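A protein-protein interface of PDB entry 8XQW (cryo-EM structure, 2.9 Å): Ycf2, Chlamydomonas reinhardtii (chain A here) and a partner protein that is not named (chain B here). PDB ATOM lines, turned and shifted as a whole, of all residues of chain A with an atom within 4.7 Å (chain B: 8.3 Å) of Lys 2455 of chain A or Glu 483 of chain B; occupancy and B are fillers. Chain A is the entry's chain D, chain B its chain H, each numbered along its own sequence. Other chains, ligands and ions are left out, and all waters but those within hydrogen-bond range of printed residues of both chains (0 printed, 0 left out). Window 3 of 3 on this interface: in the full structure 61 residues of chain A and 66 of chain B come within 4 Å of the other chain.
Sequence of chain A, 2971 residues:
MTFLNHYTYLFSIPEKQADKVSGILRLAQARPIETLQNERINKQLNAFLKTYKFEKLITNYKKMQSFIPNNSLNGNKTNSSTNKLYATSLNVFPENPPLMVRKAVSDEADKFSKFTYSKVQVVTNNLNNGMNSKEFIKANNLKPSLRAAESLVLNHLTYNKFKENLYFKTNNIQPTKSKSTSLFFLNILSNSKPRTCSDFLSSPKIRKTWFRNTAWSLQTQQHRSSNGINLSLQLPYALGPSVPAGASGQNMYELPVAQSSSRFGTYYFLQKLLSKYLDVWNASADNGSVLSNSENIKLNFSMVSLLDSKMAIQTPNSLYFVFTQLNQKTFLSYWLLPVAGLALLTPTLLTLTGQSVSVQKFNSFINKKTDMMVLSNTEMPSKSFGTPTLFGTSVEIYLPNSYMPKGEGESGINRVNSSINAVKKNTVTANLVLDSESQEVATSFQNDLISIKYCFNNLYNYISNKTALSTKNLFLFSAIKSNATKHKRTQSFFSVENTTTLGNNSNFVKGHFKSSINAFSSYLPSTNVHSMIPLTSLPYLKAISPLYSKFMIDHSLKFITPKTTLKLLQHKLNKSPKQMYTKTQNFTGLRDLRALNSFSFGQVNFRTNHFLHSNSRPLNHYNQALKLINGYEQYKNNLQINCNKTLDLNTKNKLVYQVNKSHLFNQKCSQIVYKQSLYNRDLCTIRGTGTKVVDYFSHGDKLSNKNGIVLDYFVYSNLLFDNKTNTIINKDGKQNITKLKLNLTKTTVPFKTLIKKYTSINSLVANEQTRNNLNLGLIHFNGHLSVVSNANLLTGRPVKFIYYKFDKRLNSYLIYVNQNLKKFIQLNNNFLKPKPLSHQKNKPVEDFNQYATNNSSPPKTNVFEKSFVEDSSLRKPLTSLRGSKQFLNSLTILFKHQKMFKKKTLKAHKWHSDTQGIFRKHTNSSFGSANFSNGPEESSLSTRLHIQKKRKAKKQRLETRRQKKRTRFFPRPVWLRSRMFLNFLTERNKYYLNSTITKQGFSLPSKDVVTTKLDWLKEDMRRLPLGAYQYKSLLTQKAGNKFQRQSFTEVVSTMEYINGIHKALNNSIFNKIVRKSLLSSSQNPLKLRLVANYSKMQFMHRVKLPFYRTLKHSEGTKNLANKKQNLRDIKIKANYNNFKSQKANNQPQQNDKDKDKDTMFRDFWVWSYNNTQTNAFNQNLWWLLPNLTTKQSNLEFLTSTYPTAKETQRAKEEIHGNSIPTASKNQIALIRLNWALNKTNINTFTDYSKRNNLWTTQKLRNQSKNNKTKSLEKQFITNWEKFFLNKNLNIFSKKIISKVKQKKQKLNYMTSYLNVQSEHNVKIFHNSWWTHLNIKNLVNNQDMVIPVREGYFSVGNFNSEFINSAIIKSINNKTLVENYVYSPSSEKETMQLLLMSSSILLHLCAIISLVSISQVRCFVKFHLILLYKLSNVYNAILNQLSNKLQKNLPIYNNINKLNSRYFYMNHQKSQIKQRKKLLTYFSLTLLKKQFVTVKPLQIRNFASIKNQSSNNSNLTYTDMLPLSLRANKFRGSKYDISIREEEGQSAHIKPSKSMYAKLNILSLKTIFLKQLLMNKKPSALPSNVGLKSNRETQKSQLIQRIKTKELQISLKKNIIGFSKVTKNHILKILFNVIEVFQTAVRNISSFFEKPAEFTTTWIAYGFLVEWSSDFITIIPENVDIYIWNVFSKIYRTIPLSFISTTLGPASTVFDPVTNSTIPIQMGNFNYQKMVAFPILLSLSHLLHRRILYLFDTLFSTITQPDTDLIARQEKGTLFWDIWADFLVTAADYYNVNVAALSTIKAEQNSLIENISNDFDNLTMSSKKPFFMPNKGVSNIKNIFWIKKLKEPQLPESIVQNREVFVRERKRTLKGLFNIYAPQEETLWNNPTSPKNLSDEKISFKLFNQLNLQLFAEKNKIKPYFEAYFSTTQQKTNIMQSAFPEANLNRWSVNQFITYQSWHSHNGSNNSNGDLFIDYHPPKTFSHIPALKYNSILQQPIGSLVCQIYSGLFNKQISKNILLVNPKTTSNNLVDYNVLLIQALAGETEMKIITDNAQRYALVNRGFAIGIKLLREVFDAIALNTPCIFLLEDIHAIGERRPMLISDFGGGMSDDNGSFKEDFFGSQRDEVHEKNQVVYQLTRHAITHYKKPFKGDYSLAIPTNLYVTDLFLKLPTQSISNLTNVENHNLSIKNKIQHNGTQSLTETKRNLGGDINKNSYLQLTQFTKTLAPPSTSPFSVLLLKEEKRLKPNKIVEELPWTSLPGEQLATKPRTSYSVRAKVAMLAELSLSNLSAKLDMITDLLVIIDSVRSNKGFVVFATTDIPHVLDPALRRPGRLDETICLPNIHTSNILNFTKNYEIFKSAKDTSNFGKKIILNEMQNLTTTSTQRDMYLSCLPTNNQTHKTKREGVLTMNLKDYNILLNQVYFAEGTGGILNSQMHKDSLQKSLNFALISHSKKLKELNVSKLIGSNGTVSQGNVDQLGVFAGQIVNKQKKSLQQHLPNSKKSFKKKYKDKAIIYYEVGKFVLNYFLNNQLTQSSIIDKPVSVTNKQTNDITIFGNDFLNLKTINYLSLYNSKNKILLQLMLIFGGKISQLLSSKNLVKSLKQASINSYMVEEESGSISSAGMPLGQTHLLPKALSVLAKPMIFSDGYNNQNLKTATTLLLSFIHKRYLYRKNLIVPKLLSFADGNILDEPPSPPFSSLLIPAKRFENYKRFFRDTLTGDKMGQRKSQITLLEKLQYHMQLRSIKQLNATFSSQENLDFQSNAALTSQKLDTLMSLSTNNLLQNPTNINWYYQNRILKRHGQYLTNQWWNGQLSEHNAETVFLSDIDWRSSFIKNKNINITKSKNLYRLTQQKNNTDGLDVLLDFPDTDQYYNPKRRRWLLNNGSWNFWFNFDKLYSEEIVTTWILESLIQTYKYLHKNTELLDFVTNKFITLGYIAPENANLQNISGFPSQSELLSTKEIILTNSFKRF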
ATOM      1  N   SER A2451      18.880 -20.804  14.507  1.00  0.00           N
ATOM      2  CA  SER A2451      18.736 -20.308  15.867  1.00  0.00           C
ATOM      3  C   SER A2451      18.112 -18.921  15.904  1.00  0.00           C
ATOM      4  O   SER A2451      17.394 -18.597  16.855  1.00  0.00           O
ATOM      5  CB  SER A2451      20.082 -20.309  16.576  1.00  0.00           C
ATOM      6  OG  SER A2451      21.127 -20.064  15.666  1.00  0.00           O
ATOM      7  N   HIS A2452      18.344 -18.099  14.884  1.00  0.00           N
ATOM      8  CA  HIS A2452      17.684 -16.803  14.818  1.00  0.00           C
ATOM      9  C   HIS A2452      16.178 -16.954  14.720  1.00  0.00           C
ATOM     10  O   HIS A2452      15.427 -16.245  15.398  1.00  0.00           O
ATOM     11  CB  HIS A2452      18.210 -16.024  13.625  1.00  0.00           C
ATOM     12  CG  HIS A2452      17.765 -14.602  13.590  1.00  0.00           C
ATOM     13  ND1 HIS A2452      17.108 -14.005  14.640  1.00  0.00           N
ATOM     14  CD2 HIS A2452      17.887 -13.656  12.633  1.00  0.00           C
ATOM     15  CE1 HIS A2452      16.839 -12.750  14.329  1.00  0.00           C
ATOM     16  NE2 HIS A2452      17.302 -12.512  13.117  1.00  0.00           N
ATOM     17  N   SER A2453      15.715 -17.858  13.863  1.00  0.00           N
ATOM     18  CA  SER A2453      14.276 -18.068  13.753  1.00  0.00           C
ATOM     19  C   SER A2453      13.699 -18.618  15.049  1.00  0.00           C
ATOM     20  O   SER A2453      12.571 -18.281  15.422  1.00  0.00           O
ATOM     21  CB  SER A2453      13.969 -18.992  12.589  1.00  0.00           C
ATOM     22  OG  SER A2453      14.637 -20.220  12.745  1.00  0.00           O
ATOM     23  N   LYS A2454      14.455 -19.456  15.761  1.00  0.00           N
ATOM     24  CA  LYS A2454      13.965 -19.924  17.054  1.00  0.00           C
ATOM     25  C   LYS A2454      13.849 -18.784  18.050  1.00  0.00           C
ATOM     26  O   LYS A2454      12.890 -18.726  18.826  1.00  0.00           O
ATOM     27  CB  LYS A2454      14.869 -21.010  17.616  1.00  0.00           C
ATOM     28  CG  LYS A2454      14.334 -21.609  18.890  1.00  0.00           C
ATOM     29  CD  LYS A2454      15.274 -22.651  19.433  1.00  0.00           C
ATOM     30  CE  LYS A2454      14.578 -23.603  20.368  1.00  0.00           C
ATOM     31  NZ  LYS A2454      13.776 -22.880  21.367  1.00  0.00           N
ATOM     32  N   LYS A2455      14.817 -17.874  18.052  1.00  0.00           N
ATOM     33  CA  LYS A2455      14.743 -16.723  18.942  1.00  0.00           C
ATOM     34  C   LYS A2455      13.514 -15.880  18.645  1.00  0.00           C
ATOM     35  O   LYS A2455      12.801 -15.450  19.562  1.00  0.00           O
ATOM     36  CB  LYS A2455      16.003 -15.881  18.807  1.00  0.00           C
ATOM     37  CG  LYS A2455      16.254 -14.985  19.985  1.00  0.00           C
ATOM     38  CD  LYS A2455      17.143 -13.825  19.612  1.00  0.00           C
ATOM     39  CE  LYS A2455      16.374 -12.788  18.834  1.00  0.00           C
ATOM     40  NZ  LYS A2455      17.131 -11.520  18.720  1.00  0.00           N
ATOM     41  N   LEU A2456      13.260 -15.617  17.363  1.00  0.00           N
ATOM     42  CA  LEU A2456      12.076 -14.851  16.990  1.00  0.00           C
ATOM     43  C   LEU A2456      10.804 -15.534  17.462  1.00  0.00           C
ATOM     44  O   LEU A2456       9.941 -14.897  18.071  1.00  0.00           O
ATOM     45  CB  LEU A2456      12.024 -14.647  15.480  1.00  0.00           C
ATOM     46  CG  LEU A2456      13.118 -13.785  14.875  1.00  0.00           C
ATOM     47  CD1 LEU A2456      12.836 -13.543  13.419  1.00  0.00           C
ATOM     48  CD2 LEU A2456      13.213 -12.481  15.615  1.00  0.00           C
ATOM     49  N   LYS A2457      10.664 -16.829  17.188  1.00  0.00           N
ATOM     50  CA  LYS A2457       9.451 -17.527  17.592  1.00  0.00           C
ATOM     51  C   LYS A2457       9.272 -17.495  19.101  1.00  0.00           C
ATOM     52  O   LYS A2457       8.154 -17.318  19.595  1.00  0.00           O
ATOM     53  CB  LYS A2457       9.475 -18.967  17.095  1.00  0.00           C
ATOM     54  CG  LYS A2457       8.213 -19.728  17.393  1.00  0.00           C
ATOM     55  CD  LYS A2457       7.665 -20.378  16.149  1.00  0.00           C
ATOM     56  CE  LYS A2457       6.278 -20.924  16.383  1.00  0.00           C
ATOM     57  NZ  LYS A2457       5.287 -19.841  16.562  1.00  0.00           N
ATOM     58  N   GLU A2458      10.361 -17.654  19.855  1.00  0.00           N
ATOM     59  CA  GLU A2458      10.241 -17.650  21.308  1.00  0.00           C
ATOM     60  C   GLU A2458       9.798 -16.296  21.828  1.00  0.00           C
ATOM     61  O   GLU A2458       8.810 -16.207  22.564  1.00  0.00           O
ATOM     62  CB  GLU A2458      11.560 -18.053  21.953  1.00  0.00           C
ATOM     63  CG  GLU A2458      11.912 -19.494  21.724  1.00  0.00           C
ATOM     64  CD  GLU A2458      10.711 -20.395  21.812  1.00  0.00           C
ATOM     65  OE1 GLU A2458      10.045 -20.393  22.865  1.00  0.00           O
ATOM     66  OE2 GLU A2458      10.428 -21.104  20.826  1.00  0.00           O
ATOM     67  N   LEU A2459      10.501 -15.227  21.458  1.00  0.00           N
ATOM     68  CA  LEU A2459      10.138 -13.920  21.994  1.00  0.00           C
ATOM     69  C   LEU A2459       8.784 -13.470  21.464  1.00  0.00           C
ATOM     70  O   LEU A2459       8.147 -12.583  22.036  1.00  0.00           O
ATOM     71  CB  LEU A2459      11.222 -12.884  21.688  1.00  0.00           C
ATOM     72  CG  LEU A2459      11.258 -12.105  20.370  1.00  0.00           C
ATOM     73  CD1 LEU A2459      10.350 -10.883  20.383  1.00  0.00           C
ATOM     74  CD2 LEU A2459      12.685 -11.682  20.071  1.00  0.00           C
ATOM     75  N   LEU B 143       7.696 -15.174  10.273  1.00  0.00           N
ATOM     76  CA  LEU B 143       8.285 -14.293  11.274  1.00  0.00           C
ATOM     77  C   LEU B 143       9.608 -13.722  10.795  1.00  0.00           C
ATOM     78  O   LEU B 143       9.857 -12.521  10.927  1.00  0.00           O
ATOM     79  CB  LEU B 143       8.467 -15.048  12.582  1.00  0.00           C
ATOM     80  CG  LEU B 143       7.156 -15.333  13.291  1.00  0.00           C
ATOM     81  CD1 LEU B 143       7.419 -15.985  14.606  1.00  0.00           C
ATOM     82  CD2 LEU B 143       6.411 -14.054  13.493  1.00  0.00           C
ATOM     83  N   GLU B 147      10.141  -9.764   9.933  1.00  0.00           N
ATOM     84  CA  GLU B 147      11.186  -9.056  10.651  1.00  0.00           C
ATOM     85  C   GLU B 147      12.221  -8.455   9.718  1.00  0.00           C
ATOM     86  O   GLU B 147      12.745  -7.372   9.999  1.00  0.00           O
ATOM     87  CB  GLU B 147      11.866  -9.993  11.647  1.00  0.00           C
ATOM     88  CG  GLU B 147      13.053  -9.395  12.348  1.00  0.00           C
ATOM     89  CD  GLU B 147      14.356  -9.823  11.727  1.00  0.00           C
ATOM     90  OE1 GLU B 147      14.328 -10.359  10.602  1.00  0.00           O
ATOM     91  OE2 GLU B 147      15.410  -9.628  12.364  1.00  0.00           O
ATOM     92  N   PHE B 472      13.482 -27.338  16.456  1.00  0.00           N
ATOM     93  CA  PHE B 472      14.774 -26.949  15.924  1.00  0.00           C
ATOM     94  C   PHE B 472      15.852 -27.862  16.490  1.00  0.00           C
ATOM     95  O   PHE B 472      15.778 -28.315  17.633  1.00  0.00           O
ATOM     96  CB  PHE B 472      15.057 -25.486  16.238  1.00  0.00           C
ATOM     97  CG  PHE B 472      13.905 -24.573  15.924  1.00  0.00           C
ATOM     98  CD1 PHE B 472      12.878 -24.391  16.823  1.00  0.00           C
ATOM     99  CD2 PHE B 472      13.844 -23.902  14.727  1.00  0.00           C
ATOM    100  CE1 PHE B 472      11.824 -23.565  16.530  1.00  0.00           C
ATOM    101  CE2 PHE B 472      12.791 -23.077  14.438  1.00  0.00           C
ATOM    102  CZ  PHE B 472      11.783 -22.911  15.343  1.00  0.00           C
ATOM    103  N   ALA B 476      20.170 -25.241  17.998  1.00  0.00           N
ATOM    104  CA  ALA B 476      19.464 -24.054  18.432  1.00  0.00           C
ATOM    105  C   ALA B 476      19.195 -24.065  19.922  1.00  0.00           C
ATOM    106  O   ALA B 476      18.944 -23.005  20.500  1.00  0.00           O
ATOM    107  CB  ALA B 476      18.149 -23.921  17.675  1.00  0.00           C
ATOM    108  N   ASP B 477      19.263 -25.227  20.565  1.00  0.00           N
ATOM    109  CA  ASP B 477      19.076 -25.271  22.009  1.00  0.00           C
ATOM    110  C   ASP B 477      20.229 -24.599  22.741  1.00  0.00           C
ATOM    111  O   ASP B 477      20.008 -23.851  23.699  1.00  0.00           O
ATOM    112  CB  ASP B 477      18.924 -26.713  22.472  1.00  0.00           C
ATOM    113  CG  ASP B 477      17.846 -27.446  21.723  1.00  0.00           C
ATOM    114  OD1 ASP B 477      16.960 -26.778  21.155  1.00  0.00           O
ATOM    115  OD2 ASP B 477      17.883 -28.692  21.696  1.00  0.00           O
ATOM    116  N   GLU B 478      21.465 -24.862  22.318  1.00  0.00           N
ATOM    117  CA  GLU B 478      22.605 -24.185  22.923  1.00  0.00           C
ATOM    118  C   GLU B 478      22.516 -22.683  22.721  1.00  0.00           C
ATOM    119  O   GLU B 478      22.745 -21.905  23.654  1.00  0.00           O
ATOM    120  CB  GLU B 478      23.908 -24.708  22.336  1.00  0.00           C
ATOM    121  CG  GLU B 478      24.056 -26.207  22.344  1.00  0.00           C
ATOM    122  CD  GLU B 478      25.413 -26.645  21.826  1.00  0.00           C
ATOM    123  OE1 GLU B 478      26.434 -26.220  22.401  1.00  0.00           O
ATOM    124  OE2 GLU B 478      25.463 -27.409  20.838  1.00  0.00           O
ATOM    125  N   ALA B 479      22.196 -22.254  21.505  1.00  0.00           N
ATOM    126  CA  ALA B 479      22.103 -20.825  21.243  1.00  0.00           C
ATOM    127  C   ALA B 479      21.003 -20.190  22.072  1.00  0.00           C
ATOM    128  O   ALA B 479      21.156 -19.066  22.558  1.00  0.00           O
ATOM    129  CB  ALA B 479      21.867 -20.576  19.760  1.00  0.00           C
ATOM    130  N   MET B 480      19.896 -20.898  22.275  1.00  0.00           N
ATOM    131  CA  MET B 480      18.810 -20.294  23.034  1.00  0.00           C
ATOM    132  C   MET B 480      19.089 -20.270  24.526  1.00  0.00           C
ATOM    133  O   MET B 480      18.706 -19.310  25.199  1.00  0.00           O
ATOM    134  CB  MET B 480      17.498 -21.014  22.755  1.00  0.00           C
ATOM    135  CG  MET B 480      16.731 -20.387  21.619  1.00  0.00           C
ATOM    136  SD  MET B 480      16.389 -18.653  21.905  1.00  0.00           S
ATOM    137  CE  MET B 480      15.145 -18.779  23.175  1.00  0.00           C
ATOM    138  N   GLU B 481      19.758 -21.285  25.067  1.00  0.00           N
ATOM    139  CA  GLU B 481      20.152 -21.182  26.464  1.00  0.00           C
ATOM    140  C   GLU B 481      21.186 -20.086  26.663  1.00  0.00           C
ATOM    141  O   GLU B 481      21.181 -19.421  27.699  1.00  0.00           O
ATOM    142  CB  GLU B 481      20.668 -22.520  26.987  1.00  0.00           C
ATOM    143  CG  GLU B 481      22.021 -22.942  26.463  1.00  0.00           C
ATOM    144  CD  GLU B 481      23.173 -22.359  27.253  1.00  0.00           C
ATOM    145  OE1 GLU B 481      24.327 -22.481  26.794  1.00  0.00           O
ATOM    146  OE2 GLU B 481      22.926 -21.774  28.325  1.00  0.00           O
ATOM    147  N   LEU B 482      22.062 -19.868  25.685  1.00  0.00           N
ATOM    148  CA  LEU B 482      22.972 -18.730  25.761  1.00  0.00           C
ATOM    149  C   LEU B 482      22.199 -17.420  25.770  1.00  0.00           C
ATOM    150  O   LEU B 482      22.453 -16.541  26.601  1.00  0.00           O
ATOM    151  CB  LEU B 482      23.943 -18.763  24.586  1.00  0.00           C
ATOM    152  CG  LEU B 482      25.427 -18.903  24.878  1.00  0.00           C
ATOM    153  CD1 LEU B 482      26.185 -18.888  23.578  1.00  0.00           C
ATOM    154  CD2 LEU B 482      25.874 -17.775  25.764  1.00  0.00           C
ATOM    155  N   GLU B 483      21.254 -17.271  24.842  1.00  0.00           N
ATOM    156  CA  GLU B 483      20.456 -16.054  24.774  1.00  0.00           C
ATOM    157  C   GLU B 483      19.738 -15.787  26.086  1.00  0.00           C
ATOM    158  O   GLU B 483      19.744 -14.660  26.586  1.00  0.00           O
ATOM    159  CB  GLU B 483      19.442 -16.158  23.636  1.00  0.00           C
ATOM    160  CG  GLU B 483      20.033 -15.995  22.250  1.00  0.00           C
ATOM    161  CD  GLU B 483      20.203 -14.545  21.849  1.00  0.00           C
ATOM    162  OE1 GLU B 483      20.923 -14.278  20.864  1.00  0.00           O
ATOM    163  OE2 GLU B 483      19.617 -13.671  22.519  1.00  0.00           O
ATOM    164  N   ARG B 484      19.119 -16.816  26.665  1.00  0.00           N
ATOM    165  CA  ARG B 484      18.402 -16.626  27.919  1.00  0.00           C
ATOM    166  C   ARG B 484      19.357 -16.293  29.056  1.00  0.00           C
ATOM    167  O   ARG B 484      19.191 -15.273  29.735  1.00  0.00           O
ATOM    168  CB  ARG B 484      17.584 -17.867  28.253  1.00  0.00           C
ATOM    169  CG  ARG B 484      16.207 -17.844  27.642  1.00  0.00           C
ATOM    170  CD  ARG B 484      15.304 -18.862  28.289  1.00  0.00           C
ATOM    171  NE  ARG B 484      15.764 -20.219  28.029  1.00  0.00           N
ATOM    172  CZ  ARG B 484      15.413 -20.931  26.964  1.00  0.00           C
ATOM    173  NH1 ARG B 484      14.599 -20.411  26.056  1.00  0.00           N
ATOM    174  NH2 ARG B 484      15.878 -22.161  26.810  1.00  0.00           N
ATOM    175  N   GLY B 485      20.367 -17.134  29.278  1.00  0.00           N
ATOM    176  CA  GLY B 485      21.295 -16.899  30.366  1.00  0.00           C
ATOM    177  C   GLY B 485      22.017 -15.572  30.288  1.00  0.00           C
ATOM    178  O   GLY B 485      22.436 -15.046  31.322  1.00  0.00           O
ATOM    179  N   ALA B 486      22.172 -15.014  29.091  1.00  0.00           N
ATOM    180  CA  ALA B 486      22.849 -13.731  28.966  1.00  0.00           C
ATOM    181  C   ALA B 486      21.867 -12.572  28.982  1.00  0.00           C
ATOM    182  O   ALA B 486      22.249 -11.437  29.271  1.00  0.00           O
ATOM    183  CB  ALA B 486      23.686 -13.699  27.687  1.00  0.00           C
ATOM    184  N   GLU B 487      20.605 -12.832  28.651  1.00  0.00           N
ATOM    185  CA  GLU B 487      19.589 -11.794  28.741  1.00  0.00           C
ATOM    186  C   GLU B 487      19.018 -11.677  30.145  1.00  0.00           C
ATOM    187  O   GLU B 487      18.526 -10.607  30.514  1.00  0.00           O
ATOM    188  CB  GLU B 487      18.471 -12.077  27.739  1.00  0.00           C
ATOM    189  CG  GLU B 487      17.472 -10.953  27.575  1.00  0.00           C
ATOM    190  CD  GLU B 487      16.250 -11.131  28.448  1.00  0.00           C
ATOM    191  OE1 GLU B 487      15.354 -10.263  28.403  1.00  0.00           O
ATOM    192  OE2 GLU B 487      16.189 -12.137  29.185  1.00  0.00           O
ATOM    193  N   ALA B 488      19.077 -12.743  30.933  1.00  0.00           N
ATOM    194  CA  ALA B 488      18.487 -12.765  32.262  1.00  0.00           C
ATOM    195  C   ALA B 488      19.368 -12.108  33.315  1.00  0.00           C
ATOM    196  O   ALA B 488      19.007 -12.115  34.495  1.00  0.00           O
ATOM    197  CB  ALA B 488      18.177 -14.203  32.674  1.00  0.00           C
ATOM    198  N   GLU B 489      20.510 -11.543  32.926  1.00  0.00           N
ATOM    199  CA  GLU B 489      21.356 -10.872  33.905  1.00  0.00           C
ATOM    200  C   GLU B 489      20.769  -9.524  34.309  1.00  0.00           C
ATOM    201  O   GLU B 489      21.273  -8.870  35.230  1.00  0.00           O
ATOM    202  CB  GLU B 489      22.773 -10.704  33.359  1.00  0.00           C
ATOM    203  CG  GLU B 489      22.857 -10.014  32.012  1.00  0.00           C
ATOM    204  CD  GLU B 489      22.738  -8.506  32.107  1.00  0.00           C
ATOM    205  OE1 GLU B 489      22.338  -7.876  31.109  1.00  0.00           O
ATOM    206  OE2 GLU B 489      23.044  -7.954  33.183  1.00  0.00           O
ATOM    207  N   ARG B 490      19.715  -9.088  33.630  1.00  0.00           N
ATOM    208  CA  ARG B 490      19.066  -7.823  33.951  1.00  0.00           C
ATOM    209  C   ARG B 490      17.996  -8.007  35.019  1.00  0.00           C
ATOM    210  O   ARG B 490      18.290  -8.441  36.132  1.00  0.00           O
ATOM    211  CB  ARG B 490      18.456  -7.214  32.694  1.00  0.00           C
ATOM    212  CG  ARG B 490      19.223  -7.581  31.450  1.00  0.00           C
ATOM    213  CD  ARG B 490      18.983  -6.612  30.323  1.00  0.00           C
ATOM    214  NE  ARG B 490      19.896  -6.875  29.218  1.00  0.00           N
ATOM    215  CZ  ARG B 490      19.907  -6.195  28.079  1.00  0.00           C
ATOM    216  NH1 ARG B 490      19.047  -5.205  27.885  1.00  0.00           N
ATOM    217  NH2 ARG B 490      20.778  -6.509  27.128  1.00  0.00           N
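NZ of Lys 2454 of chain A lies within salt-bridge range of OE2 of Glu 2458 of chain A.
CB of Ser 2451 of chain A touches CB of Ala 479 of chain B (3.7 Å). OE2 of Glu 147 of chain B touches NE2 of His 2452 of chain A (3.5 Å). Ser 2453 of chain A touches Phe 472 of chain B (OG to CE2, 3.8 Å). CD1 of Phe 472 of chain B touches CG of Lys 2454 of chain A, 3.8 Å away. Ala 476 of chain B touches Lys 2454 of chain A (CB to CD, 3.6 Å). Lys 2454 of chain A touches Met 480 of chain B. CA of Lys 2455 of chain A touches SD of Met 480 of chain B, 3.9 Å away. Lys 2455 of chain A touches Glu 483 of chain B (CD to OE2, 3.8 Å). CD1 of Leu 143 of chain B touches CA of Lys 2457 of chain A, at 3.9 Å. CE of Met 480 of chain B touches CG of Glu 2458 of chain A (3.6 Å).
Printed residues of chain A within 4 Å of Phe 472 of chain B: Ser 2453 (3.8 Å) and Lys 2454 (3.8 Å). Printed residues of chain B within 4 Å of Ser 2451 of chain A: Ala 479 (3.7 Å). Of the printed residues of chain A, Met 480 of chain B touches Lys 2454 (3.5 Å), Lys 2455 (3.9 Å) and Glu 2458 (3.6 Å). Arg 490 of chain B touches none of the printed residues of chain A. Ala 486 of chain B touches none of the printed residues of chain A. The nearest residue of chain B that does not touch Lys 2455 of chain A is Phe 472 of chain B (6.5 Å). The nearest printed residue of chain B that does not touch Lys 2454 of chain A is Asp 477 of chain B (4.05 Å).
Printed residues of chain A that touch a printed residue of chain B: Ser 2451, His 2452, Ser 2453, Lys 2454, Lys 2455, Lys 2457 and Glu 2458. Hydrophobic or aromatic side chains of chain B that line the printed part of chain A: Leu 143, Phe 472, Ala 476, Ala 479 and Met 480. Among the printed residues, 10 pairs touch across the chains. Among the printed residues, no Asp or Glu carboxylate lies within 4 Å of a Lys or Arg side-chain nitrogen of the other chain.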
